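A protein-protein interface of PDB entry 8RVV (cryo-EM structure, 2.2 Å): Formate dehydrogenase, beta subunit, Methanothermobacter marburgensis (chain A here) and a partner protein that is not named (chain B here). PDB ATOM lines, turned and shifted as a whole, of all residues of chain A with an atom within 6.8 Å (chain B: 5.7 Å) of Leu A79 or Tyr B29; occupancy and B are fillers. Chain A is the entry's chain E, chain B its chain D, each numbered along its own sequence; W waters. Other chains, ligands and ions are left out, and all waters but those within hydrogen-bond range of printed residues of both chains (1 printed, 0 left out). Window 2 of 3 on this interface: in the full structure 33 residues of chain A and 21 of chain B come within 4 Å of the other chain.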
ATOM      1  N   LEU A  40       9.082  23.378  -2.852  1.00  0.00           N
ATOM      2  CA  LEU A  40       7.895  23.140  -3.667  1.00  0.00           C
ATOM      3  C   LEU A  40       7.521  21.666  -3.565  1.00  0.00           C
ATOM      4  O   LEU A  40       8.296  20.799  -3.982  1.00  0.00           O
ATOM      5  CB  LEU A  40       8.146  23.537  -5.120  1.00  0.00           C
ATOM      6  CG  LEU A  40       7.007  23.276  -6.108  1.00  0.00           C
ATOM      7  CD1 LEU A  40       5.736  23.977  -5.664  1.00  0.00           C
ATOM      8  CD2 LEU A  40       7.401  23.717  -7.505  1.00  0.00           C
ATOM      9  N   LEU A  42       3.785  18.815  -2.725  1.00  0.00           N
ATOM     10  CA  LEU A  42       2.350  18.616  -2.839  1.00  0.00           C
ATOM     11  C   LEU A  42       1.704  18.618  -1.461  1.00  0.00           C
ATOM     12  O   LEU A  42       2.350  18.354  -0.445  1.00  0.00           O
ATOM     13  CB  LEU A  42       2.028  17.293  -3.548  1.00  0.00           C
ATOM     14  CG  LEU A  42       1.962  17.250  -5.075  1.00  0.00           C
ATOM     15  CD1 LEU A  42       1.177  16.023  -5.508  1.00  0.00           C
ATOM     16  CD2 LEU A  42       1.344  18.505  -5.669  1.00  0.00           C
ATOM     17  N   GLY A  51      -4.785  16.732  -5.051  1.00  0.00           N
ATOM     18  CA  GLY A  51      -3.431  17.172  -4.739  1.00  0.00           C
ATOM     19  C   GLY A  51      -3.214  18.582  -5.261  1.00  0.00           C
ATOM     20  O   GLY A  51      -3.610  18.902  -6.383  1.00  0.00           O
ATOM     21  N   ILE A  52      -2.583  19.417  -4.442  1.00  0.00           N
ATOM     22  CA  ILE A  52      -2.394  20.827  -4.767  1.00  0.00           C
ATOM     23  C   ILE A  52      -0.936  21.192  -4.520  1.00  0.00           C
ATOM     24  O   ILE A  52      -0.392  20.865  -3.456  1.00  0.00           O
ATOM     25  CB  ILE A  52      -3.340  21.714  -3.941  1.00  0.00           C
ATOM     26  CG1 ILE A  52      -4.718  21.050  -3.834  1.00  0.00           C
ATOM     27  CG2 ILE A  52      -3.444  23.097  -4.562  1.00  0.00           C
ATOM     28  CD1 ILE A  52      -5.830  21.977  -3.395  1.00  0.00           C
ATOM     29  N   PRO A  53      -0.254  21.840  -5.463  1.00  0.00           N
ATOM     30  CA  PRO A  53       1.116  22.290  -5.190  1.00  0.00           C
ATOM     31  C   PRO A  53       1.147  23.329  -4.080  1.00  0.00           C
ATOM     32  O   PRO A  53       0.274  24.192  -3.984  1.00  0.00           O
ATOM     33  CB  PRO A  53       1.575  22.878  -6.529  1.00  0.00           C
ATOM     34  CG  PRO A  53       0.643  22.322  -7.545  1.00  0.00           C
ATOM     35  CD  PRO A  53      -0.658  22.135  -6.848  1.00  0.00           C
ATOM     36  N   VAL A  54       2.170  23.240  -3.238  1.00  0.00           N
ATOM     37  CA  VAL A  54       2.379  24.180  -2.147  1.00  0.00           C
ATOM     38  C   VAL A  54       3.838  24.610  -2.145  1.00  0.00           C
ATOM     39  O   VAL A  54       4.737  23.812  -2.436  1.00  0.00           O
ATOM     40  CB  VAL A  54       1.983  23.583  -0.781  1.00  0.00           C
ATOM     41  CG1 VAL A  54       0.478  23.528  -0.647  1.00  0.00           C
ATOM     42  CG2 VAL A  54       2.588  22.203  -0.599  1.00  0.00           C
ATOM     43  N   PRO A  73      -1.238  13.246 -10.740  1.00  0.00           N
ATOM     44  CA  PRO A  73      -0.254  13.337 -11.838  1.00  0.00           C
ATOM     45  C   PRO A  73       0.114  14.784 -12.144  1.00  0.00           C
ATOM     46  O   PRO A  73      -0.263  15.369 -13.157  1.00  0.00           O
ATOM     47  CB  PRO A  73      -0.990  12.651 -12.991  1.00  0.00           C
ATOM     48  CG  PRO A  73      -2.426  12.897 -12.725  1.00  0.00           C
ATOM     49  CD  PRO A  73      -2.603  13.014 -11.238  1.00  0.00           C
ATOM     50  N   THR A  74       0.876  15.384 -11.239  1.00  0.00           N
ATOM     51  CA  THR A  74       1.228  16.792 -11.324  1.00  0.00           C
ATOM     52  C   THR A  74       2.582  16.971 -12.004  1.00  0.00           C
ATOM     53  O   THR A  74       3.383  16.041 -12.105  1.00  0.00           O
ATOM     54  CB  THR A  74       1.252  17.427  -9.931  1.00  0.00           C
ATOM     55  OG1 THR A  74       2.095  16.659  -9.064  1.00  0.00           O
ATOM     56  CG2 THR A  74      -0.154  17.482  -9.347  1.00  0.00           C
ATOM     57  N   MET A  75       2.815  18.189 -12.483  1.00  0.00           N
ATOM     58  CA  MET A  75       4.081  18.584 -13.086  1.00  0.00           C
ATOM     59  C   MET A  75       4.563  19.858 -12.409  1.00  0.00           C
ATOM     60  O   MET A  75       3.804  20.825 -12.295  1.00  0.00           O
ATOM     61  CB  MET A  75       3.929  18.797 -14.598  1.00  0.00           C
ATOM     62  CG  MET A  75       5.189  19.305 -15.305  1.00  0.00           C
ATOM     63  SD  MET A  75       6.562  18.136 -15.413  1.00  0.00           S
ATOM     64  CE  MET A  75       5.735  16.627 -15.910  1.00  0.00           C
ATOM     65  N   PHE A  76       5.819  19.856 -11.963  1.00  0.00           N
ATOM     66  CA  PHE A  76       6.396  21.000 -11.269  1.00  0.00           C
ATOM     67  C   PHE A  76       7.371  21.798 -12.122  1.00  0.00           C
ATOM     68  O   PHE A  76       7.683  22.937 -11.765  1.00  0.00           O
ATOM     69  CB  PHE A  76       7.133  20.543 -10.001  1.00  0.00           C
ATOM     70  CG  PHE A  76       6.231  20.167  -8.853  1.00  0.00           C
ATOM     71  CD1 PHE A  76       4.966  20.716  -8.715  1.00  0.00           C
ATOM     72  CD2 PHE A  76       6.665  19.266  -7.897  1.00  0.00           C
ATOM     73  CE1 PHE A  76       4.158  20.363  -7.661  1.00  0.00           C
ATOM     74  CE2 PHE A  76       5.857  18.914  -6.838  1.00  0.00           C
ATOM     75  CZ  PHE A  76       4.605  19.462  -6.722  1.00  0.00           C
ATOM     76  N   GLY A  77       7.860  21.236 -13.230  1.00  0.00           N
ATOM     77  CA  GLY A  77       8.890  21.920 -13.995  1.00  0.00           C
ATOM     78  C   GLY A  77       8.437  23.271 -14.518  1.00  0.00           C
ATOM     79  O   GLY A  77       9.134  24.278 -14.362  1.00  0.00           O
ATOM     80  N   ASP A  78       7.256  23.312 -15.133  1.00  0.00           N
ATOM     81  CA  ASP A  78       6.768  24.578 -15.668  1.00  0.00           C
ATOM     82  C   ASP A  78       6.415  25.559 -14.558  1.00  0.00           C
ATOM     83  O   ASP A  78       6.573  26.768 -14.740  1.00  0.00           O
ATOM     84  CB  ASP A  78       5.565  24.360 -16.591  1.00  0.00           C
ATOM     85  CG  ASP A  78       4.650  23.252 -16.122  1.00  0.00           C
ATOM     86  OD1 ASP A  78       4.707  22.892 -14.928  1.00  0.00           O
ATOM     87  OD2 ASP A  78       3.873  22.740 -16.954  1.00  0.00           O
ATOM     88  N   LEU A  79       5.952  25.079 -13.403  1.00  0.00           N
ATOM     89  CA  LEU A  79       5.724  25.989 -12.285  1.00  0.00           C
ATOM     90  C   LEU A  79       7.013  26.711 -11.910  1.00  0.00           C
ATOM     91  O   LEU A  79       7.037  27.940 -11.765  1.00  0.00           O
ATOM     92  CB  LEU A  79       5.172  25.222 -11.083  1.00  0.00           C
ATOM     93  CG  LEU A  79       3.657  25.031 -10.995  1.00  0.00           C
ATOM     94  CD1 LEU A  79       3.310  24.157  -9.803  1.00  0.00           C
ATOM     95  CD2 LEU A  79       2.928  26.356 -10.908  1.00  0.00           C
ATOM     96  N   ILE A  80       8.106  25.955 -11.778  1.00  0.00           N
ATOM     97  CA  ILE A  80       9.391  26.545 -11.423  1.00  0.00           C
ATOM     98  C   ILE A  80       9.846  27.514 -12.504  1.00  0.00           C
ATOM     99  O   ILE A  80      10.314  28.620 -12.215  1.00  0.00           O
ATOM    100  CB  ILE A  80      10.440  25.443 -11.188  1.00  0.00           C
ATOM    101  CG1 ILE A  80      10.066  24.591  -9.978  1.00  0.00           C
ATOM    102  CG2 ILE A  80      11.827  26.050 -11.007  1.00  0.00           C
ATOM    103  CD1 ILE A  80      10.674  23.213 -10.007  1.00  0.00           C
ATOM    104  N   SER A  81       9.725  27.112 -13.770  1.00  0.00           N
ATOM    105  CA  SER A  81      10.230  27.958 -14.845  1.00  0.00           C
ATOM    106  C   SER A  81       9.413  29.238 -14.994  1.00  0.00           C
ATOM    107  O   SER A  81       9.969  30.282 -15.346  1.00  0.00           O
ATOM    108  CB  SER A  81      10.257  27.179 -16.161  1.00  0.00           C
ATOM    109  OG  SER A  81       8.967  27.071 -16.730  1.00  0.00           O
ATOM    110  N   ARG A  82       8.108  29.190 -14.724  1.00  0.00           N
ATOM    111  CA  ARG A  82       7.241  30.345 -14.914  1.00  0.00           C
ATOM    112  C   ARG A  82       7.237  31.298 -13.726  1.00  0.00           C
ATOM    113  O   ARG A  82       7.160  32.514 -13.921  1.00  0.00           O
ATOM    114  CB  ARG A  82       5.807  29.890 -15.192  1.00  0.00           C
ATOM    115  CG  ARG A  82       5.634  29.124 -16.485  1.00  0.00           C
ATOM    116  CD  ARG A  82       4.185  29.097 -16.927  1.00  0.00           C
ATOM    117  NE  ARG A  82       3.821  27.810 -17.503  1.00  0.00           N
ATOM    118  CZ  ARG A  82       2.585  27.450 -17.820  1.00  0.00           C
ATOM    119  NH1 ARG A  82       1.557  28.262 -17.630  1.00  0.00           N
ATOM    120  NH2 ARG A  82       2.373  26.247 -18.343  1.00  0.00           N
ATOM    121  N   TYR A  83       7.312  30.787 -12.500  1.00  0.00           N
ATOM    122  CA  TYR A  83       7.126  31.636 -11.331  1.00  0.00           C
ATOM    123  C   TYR A  83       8.304  31.661 -10.374  1.00  0.00           C
ATOM    124  O   TYR A  83       8.522  32.687  -9.730  1.00  0.00           O
ATOM    125  CB  TYR A  83       5.874  31.196 -10.555  1.00  0.00           C
ATOM    126  CG  TYR A  83       4.677  30.979 -11.442  1.00  0.00           C
ATOM    127  CD1 TYR A  83       4.105  32.034 -12.139  1.00  0.00           C
ATOM    128  CD2 TYR A  83       4.126  29.716 -11.597  1.00  0.00           C
ATOM    129  CE1 TYR A  83       3.017  31.836 -12.958  1.00  0.00           C
ATOM    130  CE2 TYR A  83       3.039  29.511 -12.409  1.00  0.00           C
ATOM    131  CZ  TYR A  83       2.487  30.573 -13.087  1.00  0.00           C
ATOM    132  OH  TYR A  83       1.404  30.360 -13.900  1.00  0.00           O
ATOM    133  N   LEU A  84       9.070  30.578 -10.262  1.00  0.00           N
ATOM    134  CA  LEU A  84      10.063  30.437  -9.203  1.00  0.00           C
ATOM    135  C   LEU A  84      11.484  30.338  -9.749  1.00  0.00           C
ATOM    136  O   LEU A  84      12.366  29.802  -9.071  1.00  0.00           O
ATOM    137  CB  LEU A  84       9.739  29.212  -8.344  1.00  0.00           C
ATOM    138  CG  LEU A  84       8.261  28.991  -7.997  1.00  0.00           C
ATOM    139  CD1 LEU A  84       8.000  27.543  -7.633  1.00  0.00           C
ATOM    140  CD2 LEU A  84       7.827  29.910  -6.875  1.00  0.00           C
ATOM    141  N   SER A  85      11.731  30.851 -10.951  1.00  0.00           N
ATOM    142  CA  SER A  85      13.035  30.698 -11.585  1.00  0.00           C
ATOM    143  C   SER A  85      14.098  31.613 -10.992  1.00  0.00           C
ATOM    144  O   SER A  85      15.256  31.539 -11.419  1.00  0.00           O
ATOM    145  CB  SER A  85      12.919  30.955 -13.086  1.00  0.00           C
ATOM    146  OG  SER A  85      12.363  32.231 -13.344  1.00  0.00           O
ATOM    147  N   LEU A 104      14.360  21.949 -19.301  1.00  0.00           N
ATOM    148  CA  LEU A 104      14.290  23.397 -19.126  1.00  0.00           C
ATOM    149  C   LEU A 104      15.631  24.002 -18.713  1.00  0.00           C
ATOM    150  O   LEU A 104      15.939  25.129 -19.107  1.00  0.00           O
ATOM    151  CB  LEU A 104      13.205  23.745 -18.105  1.00  0.00           C
ATOM    152  CG  LEU A 104      11.782  23.572 -18.650  1.00  0.00           C
ATOM    153  CD1 LEU A 104      10.777  23.333 -17.536  1.00  0.00           C
ATOM    154  CD2 LEU A 104      11.382  24.774 -19.481  1.00  0.00           C
ATOM    155  N   GLN A 335       0.976  15.140 -19.901  1.00  0.00           N
ATOM    156  CA  GLN A 335       0.202  16.306 -19.489  1.00  0.00           C
ATOM    157  C   GLN A 335      -0.661  16.831 -20.631  1.00  0.00           C
ATOM    158  O   GLN A 335      -1.770  17.322 -20.396  1.00  0.00           O
ATOM    159  CB  GLN A 335       1.131  17.403 -18.970  1.00  0.00           C
ATOM    160  CG  GLN A 335       1.937  17.007 -17.746  1.00  0.00           C
ATOM    161  CD  GLN A 335       1.082  16.863 -16.507  1.00  0.00           C
ATOM    162  OE1 GLN A 335       0.180  17.661 -16.267  1.00  0.00           O
ATOM    163  NE2 GLN A 335       1.359  15.839 -15.715  1.00  0.00           N
ATOM    164  N   VAL B   2      -2.122  28.258  -4.911  1.00  0.00           N
ATOM    165  CA  VAL B   2      -3.026  27.566  -5.827  1.00  0.00           C
ATOM    166  C   VAL B   2      -4.357  27.368  -5.112  1.00  0.00           C
ATOM    167  O   VAL B   2      -4.409  26.714  -4.063  1.00  0.00           O
ATOM    168  CB  VAL B   2      -2.442  26.223  -6.291  1.00  0.00           C
ATOM    169  CG1 VAL B   2      -3.255  25.652  -7.439  1.00  0.00           C
ATOM    170  CG2 VAL B   2      -0.985  26.383  -6.689  1.00  0.00           C
ATOM    171  N   VAL B  16     -11.368  25.480 -12.143  1.00  0.00           N
ATOM    172  CA  VAL B  16      -9.991  25.848 -12.453  1.00  0.00           C
ATOM    173  C   VAL B  16      -9.278  26.132 -11.138  1.00  0.00           C
ATOM    174  O   VAL B  16      -9.907  26.272 -10.089  1.00  0.00           O
ATOM    175  CB  VAL B  16      -9.912  27.069 -13.396  1.00  0.00           C
ATOM    176  CG1 VAL B  16     -10.694  26.805 -14.662  1.00  0.00           C
ATOM    177  CG2 VAL B  16     -10.439  28.317 -12.713  1.00  0.00           C
ATOM    178  N   ASN B  17      -7.949  26.196 -11.188  1.00  0.00           N
ATOM    179  CA  ASN B  17      -7.159  26.645 -10.053  1.00  0.00           C
ATOM    180  C   ASN B  17      -6.492  27.953 -10.435  1.00  0.00           C
ATOM    181  O   ASN B  17      -5.946  28.070 -11.532  1.00  0.00           O
ATOM    182  CB  ASN B  17      -6.101  25.614  -9.662  1.00  0.00           C
ATOM    183  CG  ASN B  17      -6.678  24.430  -8.926  1.00  0.00           C
ATOM    184  OD1 ASN B  17      -7.561  24.575  -8.089  1.00  0.00           O
ATOM    185  ND2 ASN B  17      -6.179  23.249  -9.237  1.00  0.00           N
ATOM    186  N   ILE B  18      -6.539  28.930  -9.543  1.00  0.00           N
ATOM    187  CA  ILE B  18      -5.826  30.184  -9.731  1.00  0.00           C
ATOM    188  C   ILE B  18      -4.517  30.104  -8.962  1.00  0.00           C
ATOM    189  O   ILE B  18      -4.509  29.799  -7.761  1.00  0.00           O
ATOM    190  CB  ILE B  18      -6.670  31.387  -9.280  1.00  0.00           C
ATOM    191  CG1 ILE B  18      -7.815  31.612 -10.265  1.00  0.00           C
ATOM    192  CG2 ILE B  18      -5.804  32.635  -9.186  1.00  0.00           C
ATOM    193  CD1 ILE B  18      -8.852  32.601  -9.793  1.00  0.00           C
ATOM    194  N   VAL B  19      -3.414  30.332  -9.667  1.00  0.00           N
ATOM    195  CA  VAL B  19      -2.090  30.440  -9.069  1.00  0.00           C
ATOM    196  C   VAL B  19      -1.870  31.913  -8.756  1.00  0.00           C
ATOM    197  O   VAL B  19      -1.798  32.743  -9.668  1.00  0.00           O
ATOM    198  CB  VAL B  19      -0.998  29.904 -10.004  1.00  0.00           C
ATOM    199  CG1 VAL B  19       0.386  30.198  -9.433  1.00  0.00           C
ATOM    200  CG2 VAL B  19      -1.180  28.415 -10.243  1.00  0.00           C
ATOM    201  N   GLY B  27      -1.419  32.915 -12.627  1.00  0.00           N
ATOM    202  CA  GLY B  27      -1.586  31.831 -13.576  1.00  0.00           C
ATOM    203  C   GLY B  27      -2.781  30.958 -13.269  1.00  0.00           C
ATOM    204  O   GLY B  27      -3.576  31.238 -12.372  1.00  0.00           O
ATOM    205  N   THR B  28      -2.885  29.872 -14.031  1.00  0.00           N
ATOM    206  CA  THR B  28      -3.927  28.874 -13.864  1.00  0.00           C
ATOM    207  C   THR B  28      -3.284  27.500 -13.715  1.00  0.00           C
ATOM    208  O   THR B  28      -2.191  27.251 -14.227  1.00  0.00           O
ATOM    209  CB  THR B  28      -4.908  28.889 -15.059  1.00  0.00           C
ATOM    210  OG1 THR B  28      -5.874  29.932 -14.878  1.00  0.00           O
ATOM    211  CG2 THR B  28      -5.631  27.566 -15.210  1.00  0.00           C
ATOM    212  N   TYR B  29      -3.966  26.619 -12.993  1.00  0.00           N
ATOM    213  CA  TYR B  29      -3.547  25.242 -12.805  1.00  0.00           C
ATOM    214  C   TYR B  29      -4.731  24.304 -12.999  1.00  0.00           C
ATOM    215  O   TYR B  29      -5.879  24.674 -12.713  1.00  0.00           O
ATOM    216  CB  TYR B  29      -2.935  25.039 -11.410  1.00  0.00           C
ATOM    217  CG  TYR B  29      -1.945  23.902 -11.325  1.00  0.00           C
ATOM    218  CD1 TYR B  29      -0.697  23.997 -11.923  1.00  0.00           C
ATOM    219  CD2 TYR B  29      -2.257  22.735 -10.643  1.00  0.00           C
ATOM    220  CE1 TYR B  29       0.210  22.961 -11.849  1.00  0.00           C
ATOM    221  CE2 TYR B  29      -1.356  21.694 -10.562  1.00  0.00           C
ATOM    222  CZ  TYR B  29      -0.124  21.813 -11.166  1.00  0.00           C
ATOM    223  OH  TYR B  29       0.778  20.779 -11.088  1.00  0.00           O
ATOM    224  N   PRO B  30      -4.488  23.087 -13.497  1.00  0.00           N
ATOM    225  CA  PRO B  30      -5.602  22.159 -13.746  1.00  0.00           C
ATOM    226  C   PRO B  30      -6.268  21.708 -12.456  1.00  0.00           C
ATOM    227  O   PRO B  30      -5.602  21.326 -11.493  1.00  0.00           O
ATOM    228  CB  PRO B  30      -4.934  20.984 -14.472  1.00  0.00           C
ATOM    229  CG  PRO B  30      -3.696  21.536 -15.036  1.00  0.00           C
ATOM    230  CD  PRO B  30      -3.231  22.575 -14.068  1.00  0.00           C
ATOM    231  N   TYR B  31      -7.599  21.750 -12.452  1.00  0.00           N
ATOM    232  CA  TYR B  31      -8.412  21.295 -11.328  1.00  0.00           C
ATOM    233  C   TYR B  31      -8.935  19.901 -11.680  1.00  0.00           C
ATOM    234  O   TYR B  31     -10.098  19.706 -12.028  1.00  0.00           O
ATOM    235  CB  TYR B  31      -9.528  22.304 -11.059  1.00  0.00           C
ATOM    236  CG  TYR B  31     -10.351  22.083  -9.810  1.00  0.00           C
ATOM    237  CD1 TYR B  31     -10.208  20.942  -9.036  1.00  0.00           C
ATOM    238  CD2 TYR B  31     -11.290  23.024  -9.415  1.00  0.00           C
ATOM    239  CE1 TYR B  31     -10.969  20.747  -7.906  1.00  0.00           C
ATOM    240  CE2 TYR B  31     -12.057  22.838  -8.290  1.00  0.00           C
ATOM    241  CZ  TYR B  31     -11.892  21.699  -7.538  1.00  0.00           C
ATOM    242  OH  TYR B  31     -12.655  21.513  -6.413  1.00  0.00           O
ATOM    243  N   ARG B  32      -8.043  18.913 -11.569  1.00  0.00           N
ATOM    244  CA  ARG B  32      -8.332  17.574 -12.076  1.00  0.00           C
ATOM    245  C   ARG B  32      -9.485  16.912 -11.333  1.00  0.00           C
ATOM    246  O   ARG B  32     -10.173  16.054 -11.897  1.00  0.00           O
ATOM    247  CB  ARG B  32      -7.084  16.698 -11.977  1.00  0.00           C
ATOM    248  CG  ARG B  32      -6.118  16.856 -13.134  1.00  0.00           C
ATOM    249  CD  ARG B  32      -4.936  15.910 -13.012  1.00  0.00           C
ATOM    250  NE  ARG B  32      -3.982  16.089 -14.098  1.00  0.00           N
ATOM    251  CZ  ARG B  32      -3.002  16.985 -14.105  1.00  0.00           C
ATOM    252  NH1 ARG B  32      -2.802  17.801 -13.083  1.00  0.00           N
ATOM    253  NH2 ARG B  32      -2.208  17.068 -15.167  1.00  0.00           N
HETATM  254  O   HOH W   1      -0.087  19.261 -13.479  1.00  0.00           O
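The side-chain hydroxyl (OH) of Tyr B29 lies within hydrogen-bond range of the backbone carbonyl oxygen (O) of Met A75, 3.3 Å away.
NH2 of Arg B32 is in hydrogen-bond range of OE1 of Gln A335, 2.7 Å away.
The backbone carbonyl oxygen of Pro A73 lies within hydrogen-bond range of the guanidinium group of Arg B32 (3.3 Å).
Water W1 lies within hydrogen-bond range of the side-chain hydroxyl of Tyr B29, the guanidinium group of Arg B32, the side-chain amide oxygen of Gln A335 and the backbone NH of Met A75.
Among the printed residues, merely in contact across the chains: Ile A52 with Val B2 (3.7 Å), Pro A53 with Val B2 (3.7 Å), Pro A53 with Tyr B29 (3.7 Å), Thr A74 with Tyr B29 (3.6 Å), Leu A79 with Tyr B29 (3.9 Å) and Tyr A83 with Gly B27 (3.3 Å).
Hydrophobic or aromatic side chains of chain B within 4 Å of the printed part of chain A: Val B2 and Tyr B29.
Printed residues of chain A that touch a printed residue of chain B: Ile A52, Pro A53, Pro A73, Thr A74, Met A75, Leu A79, Tyr A83 and Gln A335.
Hydrophobic or aromatic side chains of chain A that line the printed part of chain B: Ile A52, Pro A53, Pro A73, Leu A79 and Tyr A83.
Of the printed residues of chain B, Pro A73 touches Arg B32.
Printed residues of chain B within 4 Å of Thr A74: Tyr B29 (3.6 Å).
Leu A79 touches just one residue of chain B: Tyr B29.
Ser A81 touches none of the printed residues of chain B.
Printed residues of chain B within 4 Å of Tyr A83: Gly B27.
Of the printed residues of chain A, Val B2 touches Ile A52 (3.7 Å) and Pro A53 (3.7 Å).
Of the printed residues of chain A, Gly B27 touches Tyr A83 (3.3 Å).
Of chain A, only Pro A53, Thr A74, Met A75 and Leu A79 come within 4 Å of Tyr B29.
The nearest residue of chain B that does not touch Leu A79 is Val B19 (4.6 Å).
The nearest residue of chain A that does not touch Tyr B29 is Phe A76 (4.8 Å).
O of Pro A73 sits at hydrogen-bond distance from NE2 of Gln A335.
The backbone carbonyl oxygen (O) of Gly B27 is in hydrogen-bond range of the backbone NH (N) of Val B19 (2.9 Å).
O of Asn B17 lies within hydrogen-bond range of N of Tyr B29 (2.9 Å).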
